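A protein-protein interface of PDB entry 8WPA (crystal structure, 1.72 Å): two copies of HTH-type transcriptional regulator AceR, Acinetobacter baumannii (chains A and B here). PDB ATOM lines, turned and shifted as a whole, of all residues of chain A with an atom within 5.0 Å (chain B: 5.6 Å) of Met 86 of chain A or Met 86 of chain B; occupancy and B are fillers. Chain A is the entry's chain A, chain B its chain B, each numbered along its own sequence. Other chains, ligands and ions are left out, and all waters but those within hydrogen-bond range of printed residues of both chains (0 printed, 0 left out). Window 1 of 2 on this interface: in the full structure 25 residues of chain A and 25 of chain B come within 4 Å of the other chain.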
ATOM      1  N   ASN A  13       5.096  14.011   3.396  1.00  0.00           N
ATOM      2  CA  ASN A  13       4.116  14.313   4.428  1.00  0.00           C
ATOM      3  C   ASN A  13       3.478  13.048   5.009  1.00  0.00           C
ATOM      4  O   ASN A  13       3.699  11.920   4.551  1.00  0.00           O
ATOM      5  CB  ASN A  13       3.059  15.276   3.883  1.00  0.00           C
ATOM      6  CG  ASN A  13       2.254  14.735   2.728  1.00  0.00           C
ATOM      7  OD1 ASN A  13       1.882  13.594   2.723  1.00  0.00           O
ATOM      8  ND2 ASN A  13       1.951  15.508   1.729  1.00  0.00           N
ATOM      9  N   GLN A  14       2.673  13.249   6.065  1.00  0.00           N
ATOM     10  CA  GLN A  14       2.082  12.148   6.802  1.00  0.00           C
ATOM     11  C   GLN A  14       1.080  11.390   5.935  1.00  0.00           C
ATOM     12  O   GLN A  14       0.997  10.178   6.010  1.00  0.00           O
ATOM     13  CB  GLN A  14       1.402  12.634   8.105  1.00  0.00           C
ATOM     14  CG  GLN A  14       0.719  11.471   8.905  1.00  0.00           C
ATOM     15  CD  GLN A  14       0.207  11.845  10.279  1.00  0.00           C
ATOM     16  OE1 GLN A  14       0.351  12.973  10.745  1.00  0.00           O
ATOM     17  NE2 GLN A  14      -0.330  10.846  10.974  1.00  0.00           N
ATOM     18  N   LEU A  17       2.763   8.757   3.898  1.00  0.00           N
ATOM     19  CA  LEU A  17       3.221   7.616   4.665  1.00  0.00           C
ATOM     20  C   LEU A  17       2.055   6.731   5.107  1.00  0.00           C
ATOM     21  O   LEU A  17       2.196   5.516   5.108  1.00  0.00           O
ATOM     22  CB  LEU A  17       4.073   8.070   5.814  1.00  0.00           C
ATOM     23  CG  LEU A  17       5.451   8.670   5.360  1.00  0.00           C
ATOM     24  CD1 LEU A  17       6.446   8.735   6.485  1.00  0.00           C
ATOM     25  CD2 LEU A  17       6.168   7.871   4.240  1.00  0.00           C
ATOM     26  N   LEU A  82       7.796   5.636  12.758  1.00  0.00           N
ATOM     27  CA  LEU A  82       7.560   7.048  12.510  1.00  0.00           C
ATOM     28  C   LEU A  82       6.062   7.355  12.483  1.00  0.00           C
ATOM     29  O   LEU A  82       5.605   8.379  12.964  1.00  0.00           O
ATOM     30  CB  LEU A  82       8.213   7.441  11.178  1.00  0.00           C
ATOM     31  CG  LEU A  82       7.912   8.839  10.661  1.00  0.00           C
ATOM     32  CD1 LEU A  82       8.256   9.904  11.637  1.00  0.00           C
ATOM     33  CD2 LEU A  82       8.677   9.123   9.405  1.00  0.00           C
ATOM     34  N   LEU A  83       5.274   6.451  11.920  1.00  0.00           N
ATOM     35  CA  LEU A  83       3.826   6.661  11.888  1.00  0.00           C
ATOM     36  C   LEU A  83       3.174   6.783  13.272  1.00  0.00           C
ATOM     37  O   LEU A  83       2.268   7.606  13.462  1.00  0.00           O
ATOM     38  CB  LEU A  83       3.222   5.538  11.020  1.00  0.00           C
ATOM     39  CG  LEU A  83       3.455   5.692   9.527  1.00  0.00           C
ATOM     40  CD1 LEU A  83       3.042   4.438   8.777  1.00  0.00           C
ATOM     41  CD2 LEU A  83       2.699   6.922   8.980  1.00  0.00           C
ATOM     42  N   ILE A  84       3.691   6.043  14.263  1.00  0.00           N
ATOM     43  CA  ILE A  84       3.228   6.209  15.629  1.00  0.00           C
ATOM     44  C   ILE A  84       3.401   7.660  16.065  1.00  0.00           C
ATOM     45  O   ILE A  84       2.479   8.311  16.562  1.00  0.00           O
ATOM     46  CB  ILE A  84       3.982   5.301  16.621  1.00  0.00           C
ATOM     47  CG1 ILE A  84       3.614   3.860  16.428  1.00  0.00           C
ATOM     48  CG2 ILE A  84       3.782   5.794  18.060  1.00  0.00           C
ATOM     49  CD1 ILE A  84       4.415   2.932  17.316  1.00  0.00           C
ATOM     50  N   GLU A  85       4.609   8.184  15.849  1.00  0.00           N
ATOM     51  CA  GLU A  85       4.911   9.524  16.321  1.00  0.00           C
ATOM     52  C   GLU A  85       4.164  10.603  15.532  1.00  0.00           C
ATOM     53  O   GLU A  85       3.785  11.620  16.102  1.00  0.00           O
ATOM     54  CB  GLU A  85       6.427   9.764  16.253  1.00  0.00           C
ATOM     55  CG  GLU A  85       7.207   8.893  17.204  1.00  0.00           C
ATOM     56  CD  GLU A  85       6.928   9.131  18.685  1.00  0.00           C
ATOM     57  OE1 GLU A  85       6.454  10.223  19.082  1.00  0.00           O
ATOM     58  OE2 GLU A  85       7.179   8.179  19.453  1.00  0.00           O
ATOM     59  N   MET A  86       3.984  10.381  14.230  1.00  0.00           N
ATOM     60  CA  MET A  86       3.203  11.301  13.419  1.00  0.00           C
ATOM     61  C   MET A  86       1.759  11.371  13.894  1.00  0.00           C
ATOM     62  O   MET A  86       1.201  12.465  13.966  1.00  0.00           O
ATOM     63  CB  MET A  86       3.205  10.888  11.947  1.00  0.00           C
ATOM     64  CG  MET A  86       4.461  11.215  11.235  1.00  0.00           C
ATOM     65  SD  MET A  86       4.395  10.494   9.581  1.00  0.00           S
ATOM     66  CE  MET A  86       5.614  11.510   8.730  1.00  0.00           C
ATOM     67  N   ASN A  87       1.180  10.218  14.270  1.00  0.00           N
ATOM     68  CA  ASN A  87      -0.186  10.235  14.760  1.00  0.00           C
ATOM     69  C   ASN A  87      -0.338  10.998  16.082  1.00  0.00           C
ATOM     70  O   ASN A  87      -1.295  11.762  16.249  1.00  0.00           O
ATOM     71  CB  ASN A  87      -0.757   8.833  14.837  1.00  0.00           C
ATOM     72  CG  ASN A  87      -2.259   8.934  15.093  1.00  0.00           C
ATOM     73  OD1 ASN A  87      -3.033   9.262  14.199  1.00  0.00           O
ATOM     74  ND2 ASN A  87      -2.649   8.830  16.299  1.00  0.00           N
ATOM     75  N   GLN A  88       0.619  10.814  16.992  1.00  0.00           N
ATOM     76  CA  GLN A  88       0.573  11.487  18.274  1.00  0.00           C
ATOM     77  C   GLN A  88       0.731  12.999  18.077  1.00  0.00           C
ATOM     78  O   GLN A  88       0.036  13.807  18.716  1.00  0.00           O
ATOM     79  CB  GLN A  88       1.685  10.981  19.232  1.00  0.00           C
ATOM     80  CG  GLN A  88       1.784   9.462  19.410  1.00  0.00           C
ATOM     81  CD  GLN A  88       1.040   8.833  20.552  1.00  0.00           C
ATOM     82  OE1 GLN A  88       0.858   7.588  20.581  1.00  0.00           O
ATOM     83  NE2 GLN A  88       0.622   9.646  21.520  1.00  0.00           N
ATOM     84  N   TRP A  89       1.658  13.375  17.187  1.00  0.00           N
ATOM     85  CA  TRP A  89       1.868  14.778  16.876  1.00  0.00           C
ATOM     86  C   TRP A  89       0.600  15.447  16.328  1.00  0.00           C
ATOM     87  O   TRP A  89       0.205  16.518  16.757  1.00  0.00           O
ATOM     88  CB  TRP A  89       3.011  14.892  15.885  1.00  0.00           C
ATOM     89  CG  TRP A  89       3.367  16.292  15.538  1.00  0.00           C
ATOM     90  CD1 TRP A  89       4.235  17.093  16.194  1.00  0.00           C
ATOM     91  CD2 TRP A  89       2.836  17.062  14.453  1.00  0.00           C
ATOM     92  NE1 TRP A  89       4.353  18.304  15.541  1.00  0.00           N
ATOM     93  CE2 TRP A  89       3.495  18.309  14.468  1.00  0.00           C
ATOM     94  CE3 TRP A  89       1.928  16.789  13.432  1.00  0.00           C
ATOM     95  CZ2 TRP A  89       3.216  19.314  13.548  1.00  0.00           C
ATOM     96  CZ3 TRP A  89       1.689  17.779  12.486  1.00  0.00           C
ATOM     97  CH2 TRP A  89       2.325  19.027  12.569  1.00  0.00           C
ATOM     98  N   LYS A  90      -0.068  14.771  15.399  1.00  0.00           N
ATOM     99  CA  LYS A  90      -1.302  15.274  14.820  1.00  0.00           C
ATOM    100  C   LYS A  90      -2.382  15.451  15.876  1.00  0.00           C
ATOM    101  O   LYS A  90      -3.149  16.414  15.833  1.00  0.00           O
ATOM    102  CB  LYS A  90      -1.788  14.323  13.723  1.00  0.00           C
ATOM    103  CG  LYS A  90      -3.095  14.744  13.086  1.00  0.00           C
ATOM    104  CD  LYS A  90      -3.362  14.028  11.814  1.00  0.00           C
ATOM    105  CE  LYS A  90      -3.797  12.622  12.044  1.00  0.00           C
ATOM    106  NZ  LYS A  90      -4.069  11.923  10.754  1.00  0.00           N
ATOM    107  N   GLN B  14       8.284  17.580   6.295  1.00  0.00           N
ATOM    108  CA  GLN B  14       9.430  17.708   7.179  1.00  0.00           C
ATOM    109  C   GLN B  14      10.071  19.087   7.039  1.00  0.00           C
ATOM    110  O   GLN B  14      10.507  19.676   8.015  1.00  0.00           O
ATOM    111  CB  GLN B  14      10.490  16.602   6.975  1.00  0.00           C
ATOM    112  CG  GLN B  14      11.581  16.705   8.063  1.00  0.00           C
ATOM    113  CD  GLN B  14      12.569  15.552   8.165  1.00  0.00           C
ATOM    114  OE1 GLN B  14      12.561  14.604   7.353  1.00  0.00           O
ATOM    115  NE2 GLN B  14      13.427  15.637   9.232  1.00  0.00           N
ATOM    116  N   LEU B  17       8.423  21.622   9.242  1.00  0.00           N
ATOM    117  CA  LEU B  17       8.730  21.403  10.652  1.00  0.00           C
ATOM    118  C   LEU B  17      10.142  21.885  10.982  1.00  0.00           C
ATOM    119  O   LEU B  17      10.343  22.503  12.014  1.00  0.00           O
ATOM    120  CB  LEU B  17       8.604  19.913  10.997  1.00  0.00           C
ATOM    121  CG  LEU B  17       7.190  19.320  10.804  1.00  0.00           C
ATOM    122  CD1 LEU B  17       7.202  17.846  11.141  1.00  0.00           C
ATOM    123  CD2 LEU B  17       6.214  20.083  11.582  1.00  0.00           C
ATOM    124  N   LEU B  82       8.757  14.471  17.597  1.00  0.00           N
ATOM    125  CA  LEU B  82       8.547  13.804  16.315  1.00  0.00           C
ATOM    126  C   LEU B  82       9.853  13.735  15.501  1.00  0.00           C
ATOM    127  O   LEU B  82      10.166  12.719  14.876  1.00  0.00           O
ATOM    128  CB  LEU B  82       7.474  14.602  15.524  1.00  0.00           C
ATOM    129  CG  LEU B  82       7.262  14.277  14.091  1.00  0.00           C
ATOM    130  CD1 LEU B  82       6.898  12.814  13.930  1.00  0.00           C
ATOM    131  CD2 LEU B  82       6.213  15.141  13.488  1.00  0.00           C
ATOM    132  N   LEU B  83      10.629  14.820  15.553  1.00  0.00           N
ATOM    133  CA  LEU B  83      11.890  14.862  14.826  1.00  0.00           C
ATOM    134  C   LEU B  83      12.919  13.861  15.302  1.00  0.00           C
ATOM    135  O   LEU B  83      13.731  13.481  14.495  1.00  0.00           O
ATOM    136  CB  LEU B  83      12.464  16.264  14.887  1.00  0.00           C
ATOM    137  CG  LEU B  83      11.788  17.283  13.966  1.00  0.00           C
ATOM    138  CD1 LEU B  83      12.316  18.664  14.181  1.00  0.00           C
ATOM    139  CD2 LEU B  83      11.948  16.883  12.444  1.00  0.00           C
ATOM    140  N   ILE B  84      12.894  13.373  16.538  1.00  0.00           N
ATOM    141  CA  ILE B  84      13.765  12.259  16.895  1.00  0.00           C
ATOM    142  C   ILE B  84      13.576  11.108  15.900  1.00  0.00           C
ATOM    143  O   ILE B  84      14.517  10.630  15.269  1.00  0.00           O
ATOM    144  CB  ILE B  84      13.537  11.732  18.305  1.00  0.00           C
ATOM    145  CG1 ILE B  84      13.951  12.729  19.355  1.00  0.00           C
ATOM    146  CG2 ILE B  84      14.271  10.381  18.470  1.00  0.00           C
ATOM    147  CD1 ILE B  84      13.589  12.300  20.715  1.00  0.00           C
ATOM    148  N   GLU B  85      12.325  10.665  15.741  1.00  0.00           N
ATOM    149  CA  GLU B  85      12.085   9.527  14.866  1.00  0.00           C
ATOM    150  C   GLU B  85      12.212   9.924  13.395  1.00  0.00           C
ATOM    151  O   GLU B  85      12.644   9.121  12.580  1.00  0.00           O
ATOM    152  CB  GLU B  85      10.738   8.904  15.196  1.00  0.00           C
ATOM    153  CG  GLU B  85      10.901   7.963  16.375  1.00  0.00           C
ATOM    154  CD  GLU B  85      11.620   6.663  16.057  1.00  0.00           C
ATOM    155  OE1 GLU B  85      11.665   6.245  14.878  1.00  0.00           O
ATOM    156  OE2 GLU B  85      12.157   6.057  17.008  1.00  0.00           O
ATOM    157  N   MET B  86      11.798  11.144  13.074  1.00  0.00           N
ATOM    158  CA  MET B  86      11.753  11.588  11.697  1.00  0.00           C
ATOM    159  C   MET B  86      13.153  11.753  11.156  1.00  0.00           C
ATOM    160  O   MET B  86      13.380  11.407  10.007  1.00  0.00           O
ATOM    161  CB  MET B  86      10.995  12.879  11.550  1.00  0.00           C
ATOM    162  CG  MET B  86      10.768  13.275  10.147  1.00  0.00           C
ATOM    163  SD  MET B  86       9.620  14.673  10.076  1.00  0.00           S
ATOM    164  CE  MET B  86       8.043  13.856  10.213  1.00  0.00           C
ATOM    165  N   ASN B  87      14.100  12.240  11.962  1.00  0.00           N
ATOM    166  CA  ASN B  87      15.469  12.379  11.467  1.00  0.00           C
ATOM    167  C   ASN B  87      16.137  11.028  11.232  1.00  0.00           C
ATOM    168  O   ASN B  87      16.856  10.870  10.231  1.00  0.00           O
ATOM    169  CB  ASN B  87      16.303  13.252  12.378  1.00  0.00           C
ATOM    170  CG  ASN B  87      15.904  14.681  12.208  1.00  0.00           C
ATOM    171  OD1 ASN B  87      15.493  15.120  11.086  1.00  0.00           O
ATOM    172  ND2 ASN B  87      15.971  15.443  13.244  1.00  0.00           N
ATOM    173  N   GLN B  88      15.861  10.064  12.132  1.00  0.00           N
ATOM    174  CA  GLN B  88      16.359   8.711  11.937  1.00  0.00           C
ATOM    175  C   GLN B  88      15.791   8.100  10.652  1.00  0.00           C
ATOM    176  O   GLN B  88      16.491   7.453   9.897  1.00  0.00           O
ATOM    177  CB  GLN B  88      16.028   7.831  13.158  1.00  0.00           C
ATOM    178  CG  GLN B  88      16.693   8.347  14.447  1.00  0.00           C
ATOM    179  CD  GLN B  88      16.352   7.552  15.684  1.00  0.00           C
ATOM    180  OE1 GLN B  88      15.750   6.481  15.604  1.00  0.00           O
ATOM    181  NE2 GLN B  88      16.711   8.055  16.896  1.00  0.00           N
ATOM    182  N   TRP B  89      14.486   8.281  10.443  1.00  0.00           N
ATOM    183  CA  TRP B  89      13.822   7.762   9.257  1.00  0.00           C
ATOM    184  C   TRP B  89      14.411   8.350   7.972  1.00  0.00           C
ATOM    185  O   TRP B  89      14.691   7.649   7.017  1.00  0.00           O
ATOM    186  CB  TRP B  89      12.317   8.047   9.338  1.00  0.00           C
ATOM    187  CG  TRP B  89      11.555   7.506   8.172  1.00  0.00           C
ATOM    188  CD1 TRP B  89      11.051   6.251   8.017  1.00  0.00           C
ATOM    189  CD2 TRP B  89      11.251   8.216   6.968  1.00  0.00           C
ATOM    190  NE1 TRP B  89      10.436   6.136   6.787  1.00  0.00           N
ATOM    191  CE2 TRP B  89      10.536   7.331   6.128  1.00  0.00           C
ATOM    192  CE3 TRP B  89      11.498   9.525   6.528  1.00  0.00           C
ATOM    193  CZ2 TRP B  89      10.051   7.717   4.885  1.00  0.00           C
ATOM    194  CZ3 TRP B  89      11.016   9.896   5.285  1.00  0.00           C
ATOM    195  CH2 TRP B  89      10.288   8.998   4.497  1.00  0.00           C
ATOM    196  N   LYS B  90      14.643   9.654   7.958  1.00  0.00           N
ATOM    197  CA  LYS B  90      15.264  10.312   6.818  1.00  0.00           C
ATOM    198  C   LYS B  90      16.647   9.731   6.515  1.00  0.00           C
ATOM    199  O   LYS B  90      16.999   9.536   5.352  1.00  0.00           O
ATOM    200  CB  LYS B  90      15.362  11.823   7.044  1.00  0.00           C
ATOM    201  CG  LYS B  90      15.908  12.528   5.820  1.00  0.00           C
ATOM    202  CD  LYS B  90      15.621  14.014   5.780  1.00  0.00           C
ATOM    203  CE  LYS B  90      16.462  14.728   6.776  1.00  0.00           C
ATOM    204  NZ  LYS B  90      16.308  16.209   6.673  1.00  0.00           N
ATOM    205  N   GLN B  91      17.418   9.424   7.569  1.00  0.00           N
ATOM    206  CA  GLN B  91      18.731   8.821   7.375  1.00  0.00           C
ATOM    207  C   GLN B  91      18.608   7.459   6.705  1.00  0.00           C
ATOM    208  O   GLN B  91      19.376   7.136   5.805  1.00  0.00           O
ATOM    209  CB  GLN B  91      19.499   8.708   8.695  1.00  0.00           C
ATOM    210  CG  GLN B  91      19.920  10.070   9.242  1.00  0.00           C
ATOM    211  CD  GLN B  91      21.029  10.024  10.282  1.00  0.00           C
ATOM    212  OE1 GLN B  91      21.394   8.971  10.819  1.00  0.00           O
ATOM    213  NE2 GLN B  91      21.567  11.195  10.578  1.00  0.00           N
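The side-chain amide oxygen (OE1) of Gln 14 of chain A lies close to the backbone carbonyl oxygen (O) of Met 86 of chain A, at 3.4 Å.
Among the printed residues, pairs that only touch across the chains: Leu 82 of chain A with Trp 89 of chain B, Trp 89 of chain A with Leu 17 of chain B, Met 86 of chain A with Met 86 of chain B, Trp 89 of chain A with Leu 82 of chain B, Met 86 of chain A with Leu 82 of chain B, Glu 85 of chain A with Leu 82 of chain B, Leu 82 of chain A with Met 86 of chain B, Glu 85 of chain A with Glu 85 of chain B, Leu 17 of chain A with Trp 89 of chain B and Leu 82 of chain A with Leu 82 of chain B.
Printed residues of chain B within 4 Å of Met 86 of chain A: Leu 82 and Met 86.
Met 86 of chain B touches two residues of chain A.
Of the printed residues of chain A, Leu 17 of chain B touches Trp 89.
Of the printed residues of chain A, Leu 82 of chain B touches Leu 82, Glu 85, Met 86 and Trp 89.
Of the printed residues of chain A, Trp 89 of chain B touches Leu 17 (3.9 Å) and Leu 82 (3.5 Å).
Printed residues of chain B within 4 Å of Glu 85 of chain A: Leu 82 (3.9 Å) and Glu 85 (3.9 Å).
Leu 83 of chain A touches none of the printed residues of chain B.
Leu 83 of chain B touches none of the printed residues of chain A.
The nearest printed residue of chain B that does not touch Met 86 of chain A is Trp 89 of chain B (6.6 Å).
The nearest printed residue of chain A that does not touch Met 86 of chain B is Glu 85 of chain A (6.4 Å).
Hydrophobic or aromatic side chains of chain B that line the printed part of chain A: Leu 17, Leu 82, Met 86 and Trp 89.
Hydrophobic or aromatic side chains of chain A that line the printed part of chain B: Leu 17, Leu 82, Met 86 and Trp 89.
Among the printed residues, 10 pairs touch across the chains.
Among the printed residues, no Asp or Glu carboxylate lies within 4 Å of a Lys or Arg side-chain nitrogen of the other chain.
Leu 17 of chain A touches Trp 89 of chain B, and with the chains exchanged Trp 89 of chain A touches Leu 17 of chain B.
Leu 82 of chain A touches Trp 89 of chain B, and with the chains exchanged Trp 89 of chain A touches Leu 82 of chain B.
Glu 85 of chain A touches Leu 82 of chain B, but with the chains exchanged Leu 82 of chain A does not touch Glu 85 of chain B (4.3 Å).
Met 86 of chain A touches its own counterpart, Met 86 of chain B.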
